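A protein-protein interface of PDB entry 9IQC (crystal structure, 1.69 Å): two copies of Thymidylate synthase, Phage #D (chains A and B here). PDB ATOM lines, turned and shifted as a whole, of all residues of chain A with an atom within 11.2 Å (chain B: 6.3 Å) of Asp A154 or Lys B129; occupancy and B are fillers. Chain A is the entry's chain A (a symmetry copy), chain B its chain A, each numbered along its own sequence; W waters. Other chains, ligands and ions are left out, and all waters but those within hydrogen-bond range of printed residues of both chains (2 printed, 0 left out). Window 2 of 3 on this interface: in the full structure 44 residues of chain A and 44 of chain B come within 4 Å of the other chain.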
ATOM      1  N   ARG A  37     -33.648 -13.649 -11.366  1.00  0.00           N
ATOM      2  CA  ARG A  37     -32.288 -13.225 -11.668  1.00  0.00           C
ATOM      3  C   ARG A  37     -31.701 -13.977 -12.856  1.00  0.00           C
ATOM      4  O   ARG A  37     -30.915 -13.406 -13.623  1.00  0.00           O
ATOM      5  CB  ARG A  37     -31.417 -13.427 -10.424  1.00  0.00           C
ATOM      6  CG  ARG A  37     -29.976 -12.961 -10.545  1.00  0.00           C
ATOM      7  CD  ARG A  37     -29.172 -13.396  -9.330  1.00  0.00           C
ATOM      8  NE  ARG A  37     -29.043 -14.850  -9.245  1.00  0.00           N
ATOM      9  CZ  ARG A  37     -28.071 -15.542  -9.823  1.00  0.00           C
ATOM     10  NH1 ARG A  37     -27.149 -14.947 -10.562  1.00  0.00           N
ATOM     11  NH2 ARG A  37     -28.015 -16.865  -9.647  1.00  0.00           N
ATOM     12  N   LYS A 104     -13.519 -11.728  -8.761  1.00  0.00           N
ATOM     13  CA  LYS A 104     -13.032 -10.707  -9.683  1.00  0.00           C
ATOM     14  C   LYS A 104     -12.878  -9.355  -8.995  1.00  0.00           C
ATOM     15  O   LYS A 104     -11.938  -8.608  -9.288  1.00  0.00           O
ATOM     16  CB  LYS A 104     -13.983 -10.593 -10.876  1.00  0.00           C
ATOM     17  CG  LYS A 104     -14.357 -11.930 -11.492  1.00  0.00           C
ATOM     18  CD  LYS A 104     -15.376 -11.771 -12.609  1.00  0.00           C
ATOM     19  CE  LYS A 104     -16.651 -11.105 -12.107  1.00  0.00           C
ATOM     20  NZ  LYS A 104     -17.709 -11.072 -13.157  1.00  0.00           N
ATOM     21  N   SER A 105     -13.787  -9.031  -8.077  1.00  0.00           N
ATOM     22  CA  SER A 105     -13.815  -7.717  -7.454  1.00  0.00           C
ATOM     23  C   SER A 105     -12.747  -7.587  -6.378  1.00  0.00           C
ATOM     24  O   SER A 105     -12.490  -8.523  -5.614  1.00  0.00           O
ATOM     25  CB  SER A 105     -15.193  -7.452  -6.846  1.00  0.00           C
ATOM     26  OG  SER A 105     -15.189  -6.267  -6.073  1.00  0.00           O
ATOM     27  N   ASP A 106     -12.129  -6.404  -6.318  1.00  0.00           N
ATOM     28  CA  ASP A 106     -11.176  -6.095  -5.259  1.00  0.00           C
ATOM     29  C   ASP A 106     -11.846  -5.969  -3.896  1.00  0.00           C
ATOM     30  O   ASP A 106     -11.150  -6.010  -2.875  1.00  0.00           O
ATOM     31  CB  ASP A 106     -10.436  -4.793  -5.581  1.00  0.00           C
ATOM     32  CG  ASP A 106      -9.549  -4.909  -6.807  1.00  0.00           C
ATOM     33  OD1 ASP A 106      -8.627  -5.753  -6.801  1.00  0.00           O
ATOM     34  OD2 ASP A 106      -9.779  -4.156  -7.779  1.00  0.00           O
ATOM     35  N   ALA A 107     -13.173  -5.818  -3.862  1.00  0.00           N
ATOM     36  CA  ALA A 107     -13.881  -5.560  -2.611  1.00  0.00           C
ATOM     37  C   ALA A 107     -13.637  -6.671  -1.594  1.00  0.00           C
ATOM     38  O   ALA A 107     -13.149  -6.423  -0.485  1.00  0.00           O
ATOM     39  CB  ALA A 107     -15.377  -5.395  -2.883  1.00  0.00           C
ATOM     40  N   LEU A 108     -13.976  -7.922  -1.961  1.00  0.00           N
ATOM     41  CA  LEU A 108     -13.751  -9.050  -1.070  1.00  0.00           C
ATOM     42  C   LEU A 108     -12.437  -9.748  -1.408  1.00  0.00           C
ATOM     43  O   LEU A 108     -11.963  -9.671  -2.546  1.00  0.00           O
ATOM     44  CB  LEU A 108     -14.911 -10.050  -1.157  1.00  0.00           C
ATOM     45  CG  LEU A 108     -15.800 -10.033  -2.403  1.00  0.00           C
ATOM     46  CD1 LEU A 108     -15.055 -10.540  -3.620  1.00  0.00           C
ATOM     47  CD2 LEU A 108     -17.051 -10.855  -2.156  1.00  0.00           C
ATOM     48  N   PHE A 112     -11.663 -15.495  -0.756  1.00  0.00           N
ATOM     49  CA  PHE A 112     -13.092 -15.633  -0.524  1.00  0.00           C
ATOM     50  C   PHE A 112     -13.682 -16.676  -1.455  1.00  0.00           C
ATOM     51  O   PHE A 112     -13.430 -16.671  -2.663  1.00  0.00           O
ATOM     52  CB  PHE A 112     -13.803 -14.290  -0.730  1.00  0.00           C
ATOM     53  CG  PHE A 112     -15.303 -14.370  -0.608  1.00  0.00           C
ATOM     54  CD1 PHE A 112     -15.922 -14.196   0.620  1.00  0.00           C
ATOM     55  CD2 PHE A 112     -16.095 -14.612  -1.722  1.00  0.00           C
ATOM     56  CE1 PHE A 112     -17.307 -14.266   0.738  1.00  0.00           C
ATOM     57  CE2 PHE A 112     -17.479 -14.687  -1.611  1.00  0.00           C
ATOM     58  CZ  PHE A 112     -18.084 -14.512  -0.379  1.00  0.00           C
ATOM     59  N   SER A 147     -24.050 -14.092   6.623  1.00  0.00           N
ATOM     60  CA  SER A 147     -24.305 -12.689   6.301  1.00  0.00           C
ATOM     61  C   SER A 147     -23.130 -12.066   5.559  1.00  0.00           C
ATOM     62  O   SER A 147     -23.332 -11.156   4.750  1.00  0.00           O
ATOM     63  CB  SER A 147     -24.636 -11.882   7.557  1.00  0.00           C
ATOM     64  OG  SER A 147     -23.524 -11.732   8.419  1.00  0.00           O
ATOM     65  N   SER A 148     -21.909 -12.558   5.783  1.00  0.00           N
ATOM     66  CA  SER A 148     -20.777 -12.038   5.021  1.00  0.00           C
ATOM     67  C   SER A 148     -20.900 -12.341   3.527  1.00  0.00           C
ATOM     68  O   SER A 148     -20.250 -11.670   2.718  1.00  0.00           O
ATOM     69  CB  SER A 148     -19.461 -12.579   5.589  1.00  0.00           C
ATOM     70  OG  SER A 148     -19.467 -13.995   5.679  1.00  0.00           O
ATOM     71  N   ASP A 149     -21.740 -13.311   3.136  1.00  0.00           N
ATOM     72  CA  ASP A 149     -22.000 -13.528   1.716  1.00  0.00           C
ATOM     73  C   ASP A 149     -22.773 -12.382   1.075  1.00  0.00           C
ATOM     74  O   ASP A 149     -22.830 -12.309  -0.160  1.00  0.00           O
ATOM     75  CB  ASP A 149     -22.773 -14.832   1.509  1.00  0.00           C
ATOM     76  CG  ASP A 149     -21.975 -16.043   1.949  1.00  0.00           C
ATOM     77  OD1 ASP A 149     -20.746 -16.050   1.708  1.00  0.00           O
ATOM     78  OD2 ASP A 149     -22.558 -16.965   2.556  1.00  0.00           O
ATOM     79  N   GLN A 150     -23.370 -11.496   1.870  1.00  0.00           N
ATOM     80  CA  GLN A 150     -24.153 -10.424   1.277  1.00  0.00           C
ATOM     81  C   GLN A 150     -23.293  -9.447   0.485  1.00  0.00           C
ATOM     82  O   GLN A 150     -23.839  -8.685  -0.319  1.00  0.00           O
ATOM     83  CB  GLN A 150     -24.952  -9.703   2.368  1.00  0.00           C
ATOM     84  CG  GLN A 150     -26.053 -10.600   2.926  1.00  0.00           C
ATOM     85  CD  GLN A 150     -26.611 -10.134   4.254  1.00  0.00           C
ATOM     86  OE1 GLN A 150     -26.489  -8.966   4.620  1.00  0.00           O
ATOM     87  NE2 GLN A 150     -27.238 -11.059   4.984  1.00  0.00           N
ATOM     88  N   ALA A 151     -21.970  -9.478   0.664  1.00  0.00           N
ATOM     89  CA  ALA A 151     -21.078  -8.701  -0.194  1.00  0.00           C
ATOM     90  C   ALA A 151     -21.210  -9.081  -1.664  1.00  0.00           C
ATOM     91  O   ALA A 151     -20.821  -8.295  -2.537  1.00  0.00           O
ATOM     92  CB  ALA A 151     -19.628  -8.881   0.259  1.00  0.00           C
ATOM     93  N   LEU A 152     -21.743 -10.268  -1.961  1.00  0.00           N
ATOM     94  CA  LEU A 152     -21.941 -10.690  -3.341  1.00  0.00           C
ATOM     95  C   LEU A 152     -23.136 -10.030  -4.007  1.00  0.00           C
ATOM     96  O   LEU A 152     -23.211 -10.030  -5.240  1.00  0.00           O
ATOM     97  CB  LEU A 152     -22.125 -12.210  -3.408  1.00  0.00           C
ATOM     98  CG  LEU A 152     -20.907 -13.074  -3.074  1.00  0.00           C
ATOM     99  CD1 LEU A 152     -21.315 -14.541  -2.949  1.00  0.00           C
ATOM    100  CD2 LEU A 152     -19.819 -12.901  -4.128  1.00  0.00           C
ATOM    101  N   LEU A 153     -24.075  -9.484  -3.229  1.00  0.00           N
ATOM    102  CA  LEU A 153     -25.369  -9.111  -3.790  1.00  0.00           C
ATOM    103  C   LEU A 153     -25.232  -8.015  -4.835  1.00  0.00           C
ATOM    104  O   LEU A 153     -25.835  -8.087  -5.910  1.00  0.00           O
ATOM    105  CB  LEU A 153     -26.317  -8.669  -2.677  1.00  0.00           C
ATOM    106  CG  LEU A 153     -26.655  -9.792  -1.698  1.00  0.00           C
ATOM    107  CD1 LEU A 153     -27.572  -9.280  -0.596  1.00  0.00           C
ATOM    108  CD2 LEU A 153     -27.281 -10.964  -2.449  1.00  0.00           C
ATOM    109  N   ASP A 154     -24.456  -6.981  -4.534  1.00  0.00           N
ATOM    110  CA  ASP A 154     -24.317  -5.860  -5.456  1.00  0.00           C
ATOM    111  C   ASP A 154     -23.019  -5.943  -6.247  1.00  0.00           C
ATOM    112  O   ASP A 154     -22.364  -4.933  -6.502  1.00  0.00           O
ATOM    113  CB  ASP A 154     -24.415  -4.544  -4.694  1.00  0.00           C
ATOM    114  CG  ASP A 154     -24.597  -3.353  -5.611  1.00  0.00           C
ATOM    115  OD1 ASP A 154     -25.367  -3.457  -6.593  1.00  0.00           O
ATOM    116  OD2 ASP A 154     -23.971  -2.313  -5.339  1.00  0.00           O
ATOM    117  N   SER A 155     -22.628  -7.144  -6.654  1.00  0.00           N
ATOM    118  CA  SER A 155     -21.404  -7.355  -7.411  1.00  0.00           C
ATOM    119  C   SER A 155     -21.722  -8.075  -8.713  1.00  0.00           C
ATOM    120  O   SER A 155     -22.836  -8.558  -8.936  1.00  0.00           O
ATOM    121  CB  SER A 155     -20.385  -8.165  -6.603  1.00  0.00           C
ATOM    122  OG  SER A 155     -20.708  -9.546  -6.646  1.00  0.00           O
ATOM    123  N   ASP A 156     -20.717  -8.151  -9.580  1.00  0.00           N
ATOM    124  CA  ASP A 156     -20.843  -8.863 -10.842  1.00  0.00           C
ATOM    125  C   ASP A 156     -20.292 -10.279 -10.757  1.00  0.00           C
ATOM    126  O   ASP A 156     -20.052 -10.910 -11.793  1.00  0.00           O
ATOM    127  CB  ASP A 156     -20.148  -8.084 -11.957  1.00  0.00           C
ATOM    128  CG  ASP A 156     -20.799  -6.741 -12.214  1.00  0.00           C
ATOM    129  OD1 ASP A 156     -22.047  -6.701 -12.313  1.00  0.00           O
ATOM    130  OD2 ASP A 156     -20.068  -5.729 -12.299  1.00  0.00           O
ATOM    131  N   GLU A 157     -20.092 -10.790  -9.544  1.00  0.00           N
ATOM    132  CA  GLU A 157     -19.499 -12.109  -9.373  1.00  0.00           C
ATOM    133  C   GLU A 157     -20.470 -13.194  -9.810  1.00  0.00           C
ATOM    134  O   GLU A 157     -21.692 -13.031  -9.752  1.00  0.00           O
ATOM    135  CB  GLU A 157     -19.098 -12.335  -7.916  1.00  0.00           C
ATOM    136  CG  GLU A 157     -18.148 -11.297  -7.353  1.00  0.00           C
ATOM    137  CD  GLU A 157     -16.742 -11.411  -7.911  1.00  0.00           C
ATOM    138  OE1 GLU A 157     -16.440 -12.409  -8.599  1.00  0.00           O
ATOM    139  OE2 GLU A 157     -15.931 -10.497  -7.652  1.00  0.00           O
ATOM    140  N   THR A 158     -19.915 -14.316 -10.260  1.00  0.00           N
ATOM    141  CA  THR A 158     -20.720 -15.471 -10.615  1.00  0.00           C
ATOM    142  C   THR A 158     -20.685 -16.550  -9.545  1.00  0.00           C
ATOM    143  O   THR A 158     -21.360 -17.571  -9.698  1.00  0.00           O
ATOM    144  CB  THR A 158     -20.263 -16.049 -11.958  1.00  0.00           C
ATOM    145  OG1 THR A 158     -18.855 -16.289 -11.919  1.00  0.00           O
ATOM    146  CG2 THR A 158     -20.566 -15.064 -13.078  1.00  0.00           C
ATOM    147  N   LEU A 159     -19.913 -16.344  -8.478  1.00  0.00           N
ATOM    148  CA  LEU A 159     -19.879 -17.282  -7.367  1.00  0.00           C
ATOM    149  C   LEU A 159     -21.276 -17.485  -6.798  1.00  0.00           C
ATOM    150  O   LEU A 159     -22.105 -16.571  -6.781  1.00  0.00           O
ATOM    151  CB  LEU A 159     -18.952 -16.778  -6.264  1.00  0.00           C
ATOM    152  CG  LEU A 159     -17.505 -16.468  -6.649  1.00  0.00           C
ATOM    153  CD1 LEU A 159     -16.667 -16.314  -5.392  1.00  0.00           C
ATOM    154  CD2 LEU A 159     -16.954 -17.561  -7.549  1.00  0.00           C
ATOM    155  N   TYR A 161     -24.070 -17.388  -4.413  1.00  0.00           N
ATOM    156  CA  TYR A 161     -24.559 -16.882  -3.141  1.00  0.00           C
ATOM    157  C   TYR A 161     -25.344 -18.033  -2.529  1.00  0.00           C
ATOM    158  O   TYR A 161     -26.395 -18.408  -3.070  1.00  0.00           O
ATOM    159  CB  TYR A 161     -25.421 -15.641  -3.368  1.00  0.00           C
ATOM    160  CG  TYR A 161     -26.108 -15.052  -2.157  1.00  0.00           C
ATOM    161  CD1 TYR A 161     -25.439 -14.177  -1.309  1.00  0.00           C
ATOM    162  CD2 TYR A 161     -27.457 -15.312  -1.905  1.00  0.00           C
ATOM    163  CE1 TYR A 161     -26.102 -13.587  -0.221  1.00  0.00           C
ATOM    164  CE2 TYR A 161     -28.111 -14.743  -0.826  1.00  0.00           C
ATOM    165  CZ  TYR A 161     -27.429 -13.888   0.014  1.00  0.00           C
ATOM    166  OH  TYR A 161     -28.093 -13.314   1.087  1.00  0.00           O
ATOM    167  N   LEU B 124     -29.443  -4.690   7.195  1.00  0.00           N
ATOM    168  CA  LEU B 124     -30.534  -3.959   6.553  1.00  0.00           C
ATOM    169  C   LEU B 124     -30.104  -3.228   5.287  1.00  0.00           C
ATOM    170  O   LEU B 124     -30.793  -3.366   4.264  1.00  0.00           O
ATOM    171  CB  LEU B 124     -31.165  -2.995   7.572  1.00  0.00           C
ATOM    172  CG  LEU B 124     -32.515  -3.441   8.132  1.00  0.00           C
ATOM    173  CD1 LEU B 124     -32.932  -2.617   9.357  1.00  0.00           C
ATOM    174  CD2 LEU B 124     -33.559  -3.356   7.032  1.00  0.00           C
ATOM    175  N   PRO B 125     -28.999  -2.467   5.269  1.00  0.00           N
ATOM    176  CA  PRO B 125     -28.662  -1.727   4.036  1.00  0.00           C
ATOM    177  C   PRO B 125     -28.489  -2.620   2.821  1.00  0.00           C
ATOM    178  O   PRO B 125     -29.101  -2.353   1.781  1.00  0.00           O
ATOM    179  CB  PRO B 125     -27.363  -1.002   4.419  1.00  0.00           C
ATOM    180  CG  PRO B 125     -27.488  -0.800   5.889  1.00  0.00           C
ATOM    181  CD  PRO B 125     -28.092  -2.096   6.374  1.00  0.00           C
ATOM    182  N   ALA B 126     -27.702  -3.702   2.936  1.00  0.00           N
ATOM    183  CA  ALA B 126     -27.472  -4.566   1.781  1.00  0.00           C
ATOM    184  C   ALA B 126     -28.734  -5.336   1.410  1.00  0.00           C
ATOM    185  O   ALA B 126     -29.038  -5.504   0.226  1.00  0.00           O
ATOM    186  CB  ALA B 126     -26.317  -5.541   2.050  1.00  0.00           C
ATOM    187  N   LEU B 127     -29.484  -5.802   2.406  1.00  0.00           N
ATOM    188  CA  LEU B 127     -30.661  -6.612   2.116  1.00  0.00           C
ATOM    189  C   LEU B 127     -31.807  -5.769   1.568  1.00  0.00           C
ATOM    190  O   LEU B 127     -32.532  -6.216   0.673  1.00  0.00           O
ATOM    191  CB  LEU B 127     -31.090  -7.367   3.369  1.00  0.00           C
ATOM    192  CG  LEU B 127     -30.100  -8.465   3.766  1.00  0.00           C
ATOM    193  CD1 LEU B 127     -30.629  -9.236   4.961  1.00  0.00           C
ATOM    194  CD2 LEU B 127     -29.801  -9.399   2.588  1.00  0.00           C
ATOM    195  N   LEU B 128     -31.982  -4.541   2.073  1.00  0.00           N
ATOM    196  CA  LEU B 128     -33.007  -3.673   1.508  1.00  0.00           C
ATOM    197  C   LEU B 128     -32.681  -3.299   0.070  1.00  0.00           C
ATOM    198  O   LEU B 128     -33.574  -3.235  -0.777  1.00  0.00           O
ATOM    199  CB  LEU B 128     -33.169  -2.407   2.347  1.00  0.00           C
ATOM    200  CG  LEU B 128     -34.142  -2.479   3.514  1.00  0.00           C
ATOM    201  CD1 LEU B 128     -34.248  -1.096   4.152  1.00  0.00           C
ATOM    202  CD2 LEU B 128     -35.511  -2.971   3.047  1.00  0.00           C
ATOM    203  N   LYS B 129     -31.410  -3.029  -0.219  1.00  0.00           N
ATOM    204  CA  LYS B 129     -31.025  -2.706  -1.587  1.00  0.00           C
ATOM    205  C   LYS B 129     -31.355  -3.854  -2.531  1.00  0.00           C
ATOM    206  O   LYS B 129     -31.961  -3.651  -3.589  1.00  0.00           O
ATOM    207  CB  LYS B 129     -29.540  -2.357  -1.640  1.00  0.00           C
ATOM    208  CG  LYS B 129     -29.055  -1.949  -3.019  1.00  0.00           C
ATOM    209  CD  LYS B 129     -27.581  -1.589  -2.985  1.00  0.00           C
ATOM    210  CE  LYS B 129     -27.066  -1.262  -4.380  1.00  0.00           C
ATOM    211  NZ  LYS B 129     -27.691  -0.028  -4.918  1.00  0.00           N
ATOM    212  N   GLU B 130     -30.979  -5.079  -2.156  1.00  0.00           N
ATOM    213  CA  GLU B 130     -31.344  -6.237  -2.962  1.00  0.00           C
ATOM    214  C   GLU B 130     -32.857  -6.341  -3.115  1.00  0.00           C
ATOM    215  O   GLU B 130     -33.375  -6.538  -4.220  1.00  0.00           O
ATOM    216  CB  GLU B 130     -30.776  -7.506  -2.324  1.00  0.00           C
ATOM    217  CG  GLU B 130     -31.205  -8.781  -3.024  1.00  0.00           C
ATOM    218  CD  GLU B 130     -30.409  -9.080  -4.285  1.00  0.00           C
ATOM    219  OE1 GLU B 130     -29.396  -8.387  -4.551  1.00  0.00           O
ATOM    220  OE2 GLU B 130     -30.804 -10.017  -5.013  1.00  0.00           O
ATOM    221  N   LEU B 131     -33.586  -6.212  -2.007  1.00  0.00           N
ATOM    222  CA  LEU B 131     -35.035  -6.388  -2.046  1.00  0.00           C
ATOM    223  C   LEU B 131     -35.700  -5.331  -2.919  1.00  0.00           C
ATOM    224  O   LEU B 131     -36.680  -5.613  -3.615  1.00  0.00           O
ATOM    225  CB  LEU B 131     -35.582  -6.346  -0.618  1.00  0.00           C
ATOM    226  CG  LEU B 131     -37.019  -6.778  -0.368  1.00  0.00           C
ATOM    227  CD1 LEU B 131     -37.310  -8.158  -0.959  1.00  0.00           C
ATOM    228  CD2 LEU B 131     -37.257  -6.775   1.127  1.00  0.00           C
ATOM    229  N   LYS B 132     -35.164  -4.113  -2.914  1.00  0.00           N
ATOM    230  CA  LYS B 132     -35.777  -3.025  -3.667  1.00  0.00           C
ATOM    231  C   LYS B 132     -35.358  -3.012  -5.131  1.00  0.00           C
ATOM    232  O   LYS B 132     -36.167  -2.660  -5.995  1.00  0.00           O
ATOM    233  CB  LYS B 132     -35.421  -1.684  -3.030  1.00  0.00           C
ATOM    234  CG  LYS B 132     -36.047  -1.443  -1.675  1.00  0.00           C
ATOM    235  CD  LYS B 132     -35.595  -0.087  -1.146  1.00  0.00           C
ATOM    236  CE  LYS B 132     -36.363   0.303   0.079  1.00  0.00           C
ATOM    237  NZ  LYS B 132     -36.024   1.701   0.484  1.00  0.00           N
ATOM    238  N   GLU B 133     -34.116  -3.403  -5.431  1.00  0.00           N
ATOM    239  CA  GLU B 133     -33.503  -3.136  -6.725  1.00  0.00           C
ATOM    240  C   GLU B 133     -33.321  -4.358  -7.610  1.00  0.00           C
ATOM    241  O   GLU B 133     -33.211  -4.198  -8.829  1.00  0.00           O
ATOM    242  CB  GLU B 133     -32.133  -2.469  -6.529  1.00  0.00           C
ATOM    243  CG  GLU B 133     -32.241  -1.084  -5.900  1.00  0.00           C
ATOM    244  CD  GLU B 133     -30.886  -0.423  -5.687  1.00  0.00           C
ATOM    245  OE1 GLU B 133     -29.872  -0.947  -6.190  1.00  0.00           O
ATOM    246  OE2 GLU B 133     -30.842   0.626  -5.013  1.00  0.00           O
ATOM    247  N   LYS B 134     -33.268  -5.564  -7.045  1.00  0.00           N
ATOM    248  CA  LYS B 134     -33.153  -6.749  -7.880  1.00  0.00           C
ATOM    249  C   LYS B 134     -34.525  -7.387  -8.004  1.00  0.00           C
ATOM    250  O   LYS B 134     -35.004  -7.998  -7.033  1.00  0.00           O
ATOM    251  CB  LYS B 134     -32.149  -7.739  -7.294  1.00  0.00           C
ATOM    252  CG  LYS B 134     -30.779  -7.122  -7.012  1.00  0.00           C
ATOM    253  CD  LYS B 134     -30.101  -6.605  -8.271  1.00  0.00           C
ATOM    254  CE  LYS B 134     -28.596  -6.406  -8.055  1.00  0.00           C
ATOM    255  NZ  LYS B 134     -28.264  -5.287  -7.127  1.00  0.00           N
HETATM  256  O   HOH W   1     -25.525  -5.199  -8.924  1.00  0.00           O
HETATM  257  O   HOH W   2     -27.804  -9.867  -6.319  1.00  0.00           O
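The side-chain amino group (NZ) of Lys B134 is in salt-bridge range of the side-chain carboxylate (OD1) of Asp A154 (3.5 Å).
NZ of Lys B129 lies within salt-bridge range of OE1 of Glu B133 (2.7 Å).
Among the printed residues, pairs that only touch across the chains: Gln A150 with Leu B127, Leu A153 with Leu B127, Leu A153 with Glu B130, Leu A153 with Lys B134 and Asp A154 with Lys B129.
Of chain B, only Lys B129 (3.4 Å) and Lys B134 (3.5 Å) come within 4 Å of Asp A154. No residue of chain A comes within 4 Å of Ala B126. No residue of chain A comes within 4 Å of Leu B128. Glu B130 touches one residue of chain A. Of the printed residues of chain B, Gln A150 touches Leu B127. Of the printed residues of chain A, Leu B127 touches Gln A150 (3.7 Å) and Leu A153 (3.9 Å). Of the printed residues of chain B, Leu A153 touches Leu B127, Glu B130 and Lys B134. Leu A152 touches none of the printed residues of chain B. The nearest residue of chain B that does not touch Asp A154 is Glu B130 (5.1 Å).
Hydrophobic or aromatic side chains of chain B that line the printed part of chain A: Leu B127. Hydrophobic or aromatic side chains of chain A within 4 Å of the printed part of chain B: Leu A153. Along chain A the printed residues that touch a printed residue of chain B span positions 150 to 154. Among the printed residues, Asp or Glu carboxylates within 4 Å of a Lys or Arg side-chain nitrogen of the other chain: Asp A154 with Lys B134 (3.5 Å).
Water W2 bridges the backbone carbonyl oxygen of Leu A153 (2.7 Å) and the side-chain carboxylate of Glu B130 (2.8 Å). Water W1 lies within hydrogen-bond range of the side-chain carboxylate of Asp A154 (2.9 Å) and the side-chain amino group of Lys B134 (3.3 Å).
No position is printed for both chains.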
